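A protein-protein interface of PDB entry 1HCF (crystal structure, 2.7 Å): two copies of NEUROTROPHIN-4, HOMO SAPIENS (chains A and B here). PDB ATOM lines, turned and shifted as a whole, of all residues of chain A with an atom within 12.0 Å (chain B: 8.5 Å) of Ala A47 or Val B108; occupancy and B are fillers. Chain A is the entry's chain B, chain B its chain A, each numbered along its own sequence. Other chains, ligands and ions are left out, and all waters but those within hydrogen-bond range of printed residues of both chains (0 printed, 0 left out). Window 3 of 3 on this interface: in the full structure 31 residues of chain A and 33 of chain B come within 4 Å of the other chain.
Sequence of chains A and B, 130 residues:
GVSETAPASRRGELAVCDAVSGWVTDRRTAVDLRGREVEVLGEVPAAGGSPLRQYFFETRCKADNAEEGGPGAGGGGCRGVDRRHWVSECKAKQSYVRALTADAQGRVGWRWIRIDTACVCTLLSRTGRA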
ATOM      1  N   GLU A  43     -27.338  10.317 -26.588  1.00  0.00           N
ATOM      2  CA  GLU A  43     -26.904   9.571 -25.418  1.00  0.00           C
ATOM      3  C   GLU A  43     -25.855  10.306 -24.591  1.00  0.00           C
ATOM      4  O   GLU A  43     -25.001  10.993 -25.135  1.00  0.00           O
ATOM      5  CB  GLU A  43     -26.389   8.200 -25.853  1.00  0.00           C
ATOM      6  CG  GLU A  43     -27.350   7.464 -26.781  1.00  0.00           C
ATOM      7  CD  GLU A  43     -26.998   5.994 -26.973  1.00  0.00           C
ATOM      8  OE1 GLU A  43     -25.823   5.681 -27.281  1.00  0.00           O
ATOM      9  OE2 GLU A  43     -27.909   5.150 -26.825  1.00  0.00           O
ATOM     10  N   VAL A  44     -25.940  10.150 -23.271  1.00  0.00           N
ATOM     11  CA  VAL A  44     -25.036  10.790 -22.311  1.00  0.00           C
ATOM     12  C   VAL A  44     -24.069   9.771 -21.688  1.00  0.00           C
ATOM     13  O   VAL A  44     -24.322   8.569 -21.755  1.00  0.00           O
ATOM     14  CB  VAL A  44     -25.878  11.498 -21.202  1.00  0.00           C
ATOM     15  CG1 VAL A  44     -27.236  10.833 -21.101  1.00  0.00           C
ATOM     16  CG2 VAL A  44     -25.188  11.422 -19.852  1.00  0.00           C
ATOM     17  N   PRO A  45     -22.942  10.239 -21.097  1.00  0.00           N
ATOM     18  CA  PRO A  45     -21.941   9.365 -20.464  1.00  0.00           C
ATOM     19  C   PRO A  45     -22.537   8.283 -19.571  1.00  0.00           C
ATOM     20  O   PRO A  45     -23.731   8.304 -19.270  1.00  0.00           O
ATOM     21  CB  PRO A  45     -21.076  10.350 -19.685  1.00  0.00           C
ATOM     22  CG  PRO A  45     -21.008  11.493 -20.628  1.00  0.00           C
ATOM     23  CD  PRO A  45     -22.464  11.636 -21.087  1.00  0.00           C
ATOM     24  N   ALA A  46     -21.701   7.346 -19.135  1.00  0.00           N
ATOM     25  CA  ALA A  46     -22.175   6.243 -18.304  1.00  0.00           C
ATOM     26  C   ALA A  46     -22.019   6.431 -16.802  1.00  0.00           C
ATOM     27  O   ALA A  46     -21.257   7.281 -16.332  1.00  0.00           O
ATOM     28  CB  ALA A  46     -21.496   4.936 -18.736  1.00  0.00           C
ATOM     29  N   ALA A  47     -22.769   5.617 -16.066  1.00  0.00           N
ATOM     30  CA  ALA A  47     -22.763   5.601 -14.609  1.00  0.00           C
ATOM     31  C   ALA A  47     -22.333   4.194 -14.195  1.00  0.00           C
ATOM     32  O   ALA A  47     -22.293   3.852 -13.010  1.00  0.00           O
ATOM     33  CB  ALA A  47     -24.162   5.894 -14.078  1.00  0.00           C
ATOM     34  N   SER A  50     -22.813   0.952 -19.674  1.00  0.00           N
ATOM     35  CA  SER A  50     -23.720   0.977 -20.819  1.00  0.00           C
ATOM     36  C   SER A  50     -24.144   2.402 -21.197  1.00  0.00           C
ATOM     37  O   SER A  50     -23.822   3.362 -20.491  1.00  0.00           O
ATOM     38  CB  SER A  50     -24.952   0.134 -20.504  1.00  0.00           C
ATOM     39  OG  SER A  50     -24.569  -1.189 -20.193  1.00  0.00           O
ATOM     40  N   PRO A  51     -24.862   2.560 -22.329  1.00  0.00           N
ATOM     41  CA  PRO A  51     -25.306   3.893 -22.759  1.00  0.00           C
ATOM     42  C   PRO A  51     -26.208   4.577 -21.730  1.00  0.00           C
ATOM     43  O   PRO A  51     -26.011   4.430 -20.522  1.00  0.00           O
ATOM     44  CB  PRO A  51     -26.042   3.609 -24.070  1.00  0.00           C
ATOM     45  CG  PRO A  51     -25.314   2.414 -24.610  1.00  0.00           C
ATOM     46  CD  PRO A  51     -25.148   1.555 -23.372  1.00  0.00           C
ATOM     47  N   LEU A  52     -27.195   5.321 -22.226  1.00  0.00           N
ATOM     48  CA  LEU A  52     -28.160   6.051 -21.398  1.00  0.00           C
ATOM     49  C   LEU A  52     -28.721   7.188 -22.253  1.00  0.00           C
ATOM     50  O   LEU A  52     -28.058   8.209 -22.434  1.00  0.00           O
ATOM     51  CB  LEU A  52     -27.476   6.640 -20.156  1.00  0.00           C
ATOM     52  CG  LEU A  52     -28.380   7.020 -18.978  1.00  0.00           C
ATOM     53  CD1 LEU A  52     -28.749   5.756 -18.203  1.00  0.00           C
ATOM     54  CD2 LEU A  52     -27.668   8.017 -18.065  1.00  0.00           C
ATOM     55  N   ARG A  53     -29.933   7.014 -22.779  1.00  0.00           N
ATOM     56  CA  ARG A  53     -30.536   8.039 -23.623  1.00  0.00           C
ATOM     57  C   ARG A  53     -30.689   9.360 -22.888  1.00  0.00           C
ATOM     58  O   ARG A  53     -31.088   9.398 -21.725  1.00  0.00           O
ATOM     59  CB  ARG A  53     -31.898   7.583 -24.167  1.00  0.00           C
ATOM     60  CG  ARG A  53     -32.951   7.356 -23.125  1.00  0.00           C
ATOM     61  N   GLN A  54     -30.346  10.444 -23.575  1.00  0.00           N
ATOM     62  CA  GLN A  54     -30.447  11.767 -22.995  1.00  0.00           C
ATOM     63  C   GLN A  54     -31.811  12.346 -23.328  1.00  0.00           C
ATOM     64  O   GLN A  54     -32.208  12.383 -24.491  1.00  0.00           O
ATOM     65  CB  GLN A  54     -29.345  12.686 -23.544  1.00  0.00           C
ATOM     66  CG  GLN A  54     -29.278  14.055 -22.853  1.00  0.00           C
ATOM     67  CD  GLN A  54     -28.099  14.915 -23.307  1.00  0.00           C
ATOM     68  OE1 GLN A  54     -27.660  15.802 -22.588  1.00  0.00           O
ATOM     69  NE2 GLN A  54     -27.597  14.657 -24.503  1.00  0.00           N
ATOM     70  N   LEU A 100     -25.089  17.094 -23.060  1.00  0.00           N
ATOM     71  CA  LEU A 100     -24.032  16.592 -23.937  1.00  0.00           C
ATOM     72  C   LEU A 100     -24.451  17.043 -25.337  1.00  0.00           C
ATOM     73  O   LEU A 100     -25.482  16.632 -25.864  1.00  0.00           O
ATOM     74  CB  LEU A 100     -23.955  15.076 -23.857  1.00  0.00           C
ATOM     75  CG  LEU A 100     -22.745  14.467 -24.558  1.00  0.00           C
ATOM     76  CD1 LEU A 100     -21.482  14.949 -23.859  1.00  0.00           C
ATOM     77  CD2 LEU A 100     -22.842  12.945 -24.527  1.00  0.00           C
ATOM     78  N   TRP A 110     -20.262  18.981 -22.828  1.00  0.00           N
ATOM     79  CA  TRP A 110     -21.393  19.407 -22.014  1.00  0.00           C
ATOM     80  C   TRP A 110     -21.596  20.891 -22.235  1.00  0.00           C
ATOM     81  O   TRP A 110     -20.633  21.656 -22.250  1.00  0.00           O
ATOM     82  CB  TRP A 110     -21.123  19.195 -20.533  1.00  0.00           C
ATOM     83  CG  TRP A 110     -21.087  17.783 -20.124  1.00  0.00           C
ATOM     84  CD1 TRP A 110     -19.985  17.015 -19.945  1.00  0.00           C
ATOM     85  CD2 TRP A 110     -22.215  16.942 -19.879  1.00  0.00           C
ATOM     86  NE1 TRP A 110     -20.349  15.741 -19.603  1.00  0.00           N
ATOM     87  CE2 TRP A 110     -21.716  15.667 -19.556  1.00  0.00           C
ATOM     88  CE3 TRP A 110     -23.599  17.142 -19.903  1.00  0.00           C
ATOM     89  CZ2 TRP A 110     -22.554  14.589 -19.258  1.00  0.00           C
ATOM     90  CZ3 TRP A 110     -24.432  16.078 -19.610  1.00  0.00           C
ATOM     91  CH2 TRP A 110     -23.908  14.815 -19.292  1.00  0.00           C
ATOM     92  N   GLU B  39     -27.144  11.822  -2.427  1.00  0.00           N
ATOM     93  CA  GLU B  39     -25.888  12.550  -2.409  1.00  0.00           C
ATOM     94  C   GLU B  39     -25.595  13.012  -3.836  1.00  0.00           C
ATOM     95  O   GLU B  39     -25.750  12.247  -4.784  1.00  0.00           O
ATOM     96  CB  GLU B  39     -24.772  11.621  -1.928  1.00  0.00           C
ATOM     97  CG  GLU B  39     -23.427  12.290  -1.785  1.00  0.00           C
ATOM     98  CD  GLU B  39     -23.345  13.170  -0.553  1.00  0.00           C
ATOM     99  OE1 GLU B  39     -22.419  14.017  -0.475  1.00  0.00           O
ATOM    100  OE2 GLU B  39     -24.203  13.002   0.343  1.00  0.00           O
ATOM    101  N   LEU B  41     -22.769  14.156  -6.358  1.00  0.00           N
ATOM    102  CA  LEU B  41     -21.323  14.179  -6.527  1.00  0.00           C
ATOM    103  C   LEU B  41     -20.774  15.517  -7.023  1.00  0.00           C
ATOM    104  O   LEU B  41     -21.479  16.300  -7.649  1.00  0.00           O
ATOM    105  CB  LEU B  41     -20.895  13.040  -7.451  1.00  0.00           C
ATOM    106  CG  LEU B  41     -20.726  11.667  -6.778  1.00  0.00           C
ATOM    107  CD1 LEU B  41     -21.942  11.316  -5.945  1.00  0.00           C
ATOM    108  CD2 LEU B  41     -20.488  10.620  -7.844  1.00  0.00           C
ATOM    109  N   GLU B  43     -18.327  15.912  -9.206  1.00  0.00           N
ATOM    110  CA  GLU B  43     -17.830  15.899 -10.571  1.00  0.00           C
ATOM    111  C   GLU B  43     -18.505  14.873 -11.469  1.00  0.00           C
ATOM    112  O   GLU B  43     -18.938  13.823 -11.019  1.00  0.00           O
ATOM    113  CB  GLU B  43     -16.296  15.746 -10.602  1.00  0.00           C
ATOM    114  CG  GLU B  43     -15.725  14.536  -9.908  1.00  0.00           C
ATOM    115  CD  GLU B  43     -14.207  14.604  -9.780  1.00  0.00           C
ATOM    116  OE1 GLU B  43     -13.618  13.648  -9.237  1.00  0.00           O
ATOM    117  OE2 GLU B  43     -13.604  15.613 -10.214  1.00  0.00           O
ATOM    118  N   PRO B  45     -18.331  12.833 -15.444  1.00  0.00           N
ATOM    119  CA  PRO B  45     -17.334  12.416 -16.436  1.00  0.00           C
ATOM    120  C   PRO B  45     -17.401  13.362 -17.635  1.00  0.00           C
ATOM    121  O   PRO B  45     -18.475  13.588 -18.197  1.00  0.00           O
ATOM    122  CB  PRO B  45     -17.770  10.995 -16.775  1.00  0.00           C
ATOM    123  CG  PRO B  45     -19.268  11.082 -16.656  1.00  0.00           C
ATOM    124  CD  PRO B  45     -19.438  11.864 -15.371  1.00  0.00           C
ATOM    125  N   ALA B  99     -28.686  14.257 -12.534  1.00  0.00           N
ATOM    126  CA  ALA B  99     -27.461  14.540 -11.804  1.00  0.00           C
ATOM    127  C   ALA B  99     -26.748  13.259 -11.425  1.00  0.00           C
ATOM    128  O   ALA B  99     -27.398  12.226 -11.227  1.00  0.00           O
ATOM    129  CB  ALA B  99     -27.776  15.353 -10.562  1.00  0.00           C
ATOM    130  N   LEU B 100     -25.418  13.321 -11.344  1.00  0.00           N
ATOM    131  CA  LEU B 100     -24.645  12.148 -10.961  1.00  0.00           C
ATOM    132  C   LEU B 100     -24.753  12.084  -9.450  1.00  0.00           C
ATOM    133  O   LEU B 100     -24.321  12.993  -8.742  1.00  0.00           O
ATOM    134  CB  LEU B 100     -23.191  12.274 -11.408  1.00  0.00           C
ATOM    135  CG  LEU B 100     -22.308  11.037 -11.187  1.00  0.00           C
ATOM    136  CD1 LEU B 100     -23.147   9.770 -11.107  1.00  0.00           C
ATOM    137  CD2 LEU B 100     -21.310  10.940 -12.329  1.00  0.00           C
ATOM    138  N   THR B 101     -25.349  11.008  -8.957  1.00  0.00           N
ATOM    139  CA  THR B 101     -25.577  10.891  -7.531  1.00  0.00           C
ATOM    140  C   THR B 101     -25.285   9.529  -6.930  1.00  0.00           C
ATOM    141  O   THR B 101     -24.946   8.576  -7.624  1.00  0.00           O
ATOM    142  CB  THR B 101     -27.026  11.235  -7.220  1.00  0.00           C
ATOM    143  OG1 THR B 101     -27.871  10.322  -7.922  1.00  0.00           O
ATOM    144  CG2 THR B 101     -27.354  12.665  -7.664  1.00  0.00           C
ATOM    145  N   ALA B 102     -25.427   9.462  -5.614  1.00  0.00           N
ATOM    146  CA  ALA B 102     -25.202   8.245  -4.866  1.00  0.00           C
ATOM    147  C   ALA B 102     -26.341   8.141  -3.868  1.00  0.00           C
ATOM    148  O   ALA B 102     -26.639   9.111  -3.185  1.00  0.00           O
ATOM    149  CB  ALA B 102     -23.885   8.334  -4.149  1.00  0.00           C
ATOM    150  N   ASP B 103     -26.980   6.978  -3.782  1.00  0.00           N
ATOM    151  CA  ASP B 103     -28.096   6.792  -2.853  1.00  0.00           C
ATOM    152  C   ASP B 103     -27.678   6.359  -1.442  1.00  0.00           C
ATOM    153  O   ASP B 103     -26.494   6.131  -1.164  1.00  0.00           O
ATOM    154  CB  ASP B 103     -29.087   5.771  -3.407  1.00  0.00           C
ATOM    155  CG  ASP B 103     -28.523   4.363  -3.439  1.00  0.00           C
ATOM    156  OD1 ASP B 103     -29.278   3.438  -3.803  1.00  0.00           O
ATOM    157  OD2 ASP B 103     -27.334   4.174  -3.107  1.00  0.00           O
ATOM    158  N   ALA B 104     -28.675   6.246  -0.563  1.00  0.00           N
ATOM    159  CA  ALA B 104     -28.485   5.849   0.835  1.00  0.00           C
ATOM    160  C   ALA B 104     -27.452   4.740   1.003  1.00  0.00           C
ATOM    161  O   ALA B 104     -26.549   4.846   1.833  1.00  0.00           O
ATOM    162  CB  ALA B 104     -29.820   5.407   1.439  1.00  0.00           C
ATOM    163  N   GLN B 105     -27.593   3.680   0.218  1.00  0.00           N
ATOM    164  CA  GLN B 105     -26.666   2.563   0.282  1.00  0.00           C
ATOM    165  C   GLN B 105     -25.289   3.055  -0.140  1.00  0.00           C
ATOM    166  O   GLN B 105     -24.427   3.296   0.705  1.00  0.00           O
ATOM    167  CB  GLN B 105     -27.132   1.432  -0.644  1.00  0.00           C
ATOM    168  CG  GLN B 105     -28.422   0.748  -0.207  1.00  0.00           C
ATOM    169  CD  GLN B 105     -29.537   1.734   0.118  1.00  0.00           C
ATOM    170  OE1 GLN B 105     -29.509   2.404   1.154  1.00  0.00           O
ATOM    171  NE2 GLN B 105     -30.521   1.832  -0.772  1.00  0.00           N
ATOM    172  N   GLY B 106     -25.090   3.209  -1.448  1.00  0.00           N
ATOM    173  CA  GLY B 106     -23.813   3.677  -1.956  1.00  0.00           C
ATOM    174  C   GLY B 106     -23.735   3.643  -3.470  1.00  0.00           C
ATOM    175  O   GLY B 106     -22.727   4.036  -4.065  1.00  0.00           O
ATOM    176  N   ARG B 107     -24.811   3.175  -4.093  1.00  0.00           N
ATOM    177  CA  ARG B 107     -24.886   3.069  -5.547  1.00  0.00           C
ATOM    178  C   ARG B 107     -24.810   4.430  -6.248  1.00  0.00           C
ATOM    179  O   ARG B 107     -25.666   5.298  -6.053  1.00  0.00           O
ATOM    180  CB  ARG B 107     -26.172   2.333  -5.946  1.00  0.00           C
ATOM    181  CG  ARG B 107     -26.149   0.818  -5.703  1.00  0.00           C
ATOM    182  N   VAL B 108     -23.767   4.604  -7.058  1.00  0.00           N
ATOM    183  CA  VAL B 108     -23.535   5.839  -7.798  1.00  0.00           C
ATOM    184  C   VAL B 108     -24.208   5.745  -9.153  1.00  0.00           C
ATOM    185  O   VAL B 108     -24.279   4.663  -9.735  1.00  0.00           O
ATOM    186  CB  VAL B 108     -22.022   6.079  -8.000  1.00  0.00           C
ATOM    187  CG1 VAL B 108     -21.790   7.173  -9.019  1.00  0.00           C
ATOM    188  CG2 VAL B 108     -21.378   6.443  -6.674  1.00  0.00           C
ATOM    189  N   GLY B 109     -24.701   6.877  -9.652  1.00  0.00           N
ATOM    190  CA  GLY B 109     -25.370   6.890 -10.943  1.00  0.00           C
ATOM    191  C   GLY B 109     -26.251   8.101 -11.208  1.00  0.00           C
ATOM    192  O   GLY B 109     -26.489   8.929 -10.325  1.00  0.00           O
ATOM    193  N   TRP B 110     -26.735   8.201 -12.444  1.00  0.00           N
ATOM    194  CA  TRP B 110     -27.594   9.311 -12.861  1.00  0.00           C
ATOM    195  C   TRP B 110     -29.035   9.178 -12.386  1.00  0.00           C
ATOM    196  O   TRP B 110     -29.711   8.199 -12.691  1.00  0.00           O
ATOM    197  CB  TRP B 110     -27.603   9.438 -14.381  1.00  0.00           C
ATOM    198  CG  TRP B 110     -26.288   9.810 -14.973  1.00  0.00           C
ATOM    199  CD1 TRP B 110     -25.388   8.973 -15.563  1.00  0.00           C
ATOM    200  CD2 TRP B 110     -25.738  11.129 -15.076  1.00  0.00           C
ATOM    201  NE1 TRP B 110     -24.316   9.689 -16.036  1.00  0.00           N
ATOM    202  CE2 TRP B 110     -24.504  11.015 -15.751  1.00  0.00           C
ATOM    203  CE3 TRP B 110     -26.168  12.397 -14.665  1.00  0.00           C
ATOM    204  CZ2 TRP B 110     -23.695  12.123 -16.029  1.00  0.00           C
ATOM    205  CZ3 TRP B 110     -25.363  13.498 -14.941  1.00  0.00           C
ATOM    206  CH2 TRP B 110     -24.139  13.352 -15.617  1.00  0.00           C
ATOM    207  N   ARG B 111     -29.496  10.179 -11.645  1.00  0.00           N
ATOM    208  CA  ARG B 111     -30.852  10.198 -11.135  1.00  0.00           C
ATOM    209  C   ARG B 111     -31.489  11.557 -11.372  1.00  0.00           C
ATOM    210  O   ARG B 111     -30.792  12.563 -11.552  1.00  0.00           O
ATOM    211  CB  ARG B 111     -30.864   9.889  -9.640  1.00  0.00           C
ATOM    212  CG  ARG B 111     -30.367   8.487  -9.282  1.00  0.00           C
ATOM    213  CD  ARG B 111     -30.642   8.169  -7.816  1.00  0.00           C
ATOM    214  NE  ARG B 111     -29.987   6.945  -7.361  1.00  0.00           N
ATOM    215  CZ  ARG B 111     -28.670   6.802  -7.223  1.00  0.00           C
ATOM    216  NH1 ARG B 111     -27.846   7.806  -7.504  1.00  0.00           N
ATOM    217  NH2 ARG B 111     -28.172   5.656  -6.794  1.00  0.00           N
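Of chain B, only Val B108 (3.9 Å), Gly B109 (3.5 Å) and Trp B110 (3.6 Å) come within 4 Å of Ala A47.
Of chain A, only Ala A47 (3.9 Å) comes within 4 Å of Val B108.
Of chain B, only Trp B110 (3.9 Å) comes within 4 Å of Ala A46.
No residue of chain A comes within 4 Å of Leu B100.
No residue of chain A comes within 4 Å of Thr B101.
No residue of chain A comes within 4 Å of Gly B106.
No residue of chain A comes within 4 Å of Arg B107.
Trp B110 touches just these residues of chain A: Pro A45 (3.6 Å), Ala A46 (3.9 Å), Ala A47 (3.6 Å), Leu A52 (3.5 Å) and Trp A110 (3.96 Å).
Of the printed residues of chain B, Leu A52 touches Trp B110 (3.5 Å).
Of the printed residues of chain B, Pro A45 touches Pro B45 and Trp B110.
Of the printed residues of chain B, Trp A110 touches Pro B45 and Trp B110.
Leu B41 touches none of the printed residues of chain A.
Arg A53 touches none of the printed residues of chain B.
The nearest residue of chain B that does not touch Ala A47 is Leu B100 (5.0 Å).
The nearest residue of chain A that does not touch Val B108 is Ala A46 (7.3 Å).
The nearest printed residue of chain A that does not touch Pro B45 is Ala A46 (4.3 Å).
O of Pro B45 is in hydrogen-bond range of NE1 of Trp A110, at 3.2 Å.
Among the printed residues, merely in contact across the chains: Ala A47 with Gly B109, Leu A52 with Trp B110, Pro A45 with Trp B110, Pro A45 with Pro B45, Ala A47 with Trp B110, Ala A46 with Trp B110, Ala A47 with Val B108 and Trp A110 with Trp B110.
Pro A45 touches its own counterpart, Pro B45.
Pro A45 touches Trp B110, and with the chains exchanged Trp A110 touches Pro B45.
Trp A110 touches its own counterpart, Trp B110.
4 positions are printed for both chains.
Of the 9 pairs that touch across the chains among the printed residues, 4 have their exchanged pair printed and touching as well.
Printed residues of chain A that touch a printed residue of chain B: Pro A45, Ala A46, Ala A47, Leu A52 and Trp A110.
Hydrophobic or aromatic side chains of chain A that line the printed part of chain B: Pro A45, Ala A47, Leu A52 and Trp A110.
Along chain A the printed residues that touch a printed residue of chain B span positions 45 to 110.
Of the 17 printed residues of chain B, 4 touch a printed residue of chain A.
The backbone carbonyl oxygen (O) of Thr B101 is in hydrogen-bond range of the backbone NH (N) of Gly B109, 2.7 Å away.
The backbone carbonyl oxygen of Gly B109 lies within hydrogen-bond range of the guanidinium group of Arg B111 (3.3 Å).
The backbone NH (N) of Val A44 sits at hydrogen-bond distance from the backbone carbonyl oxygen (O) of Leu A52 (3.0 Å).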
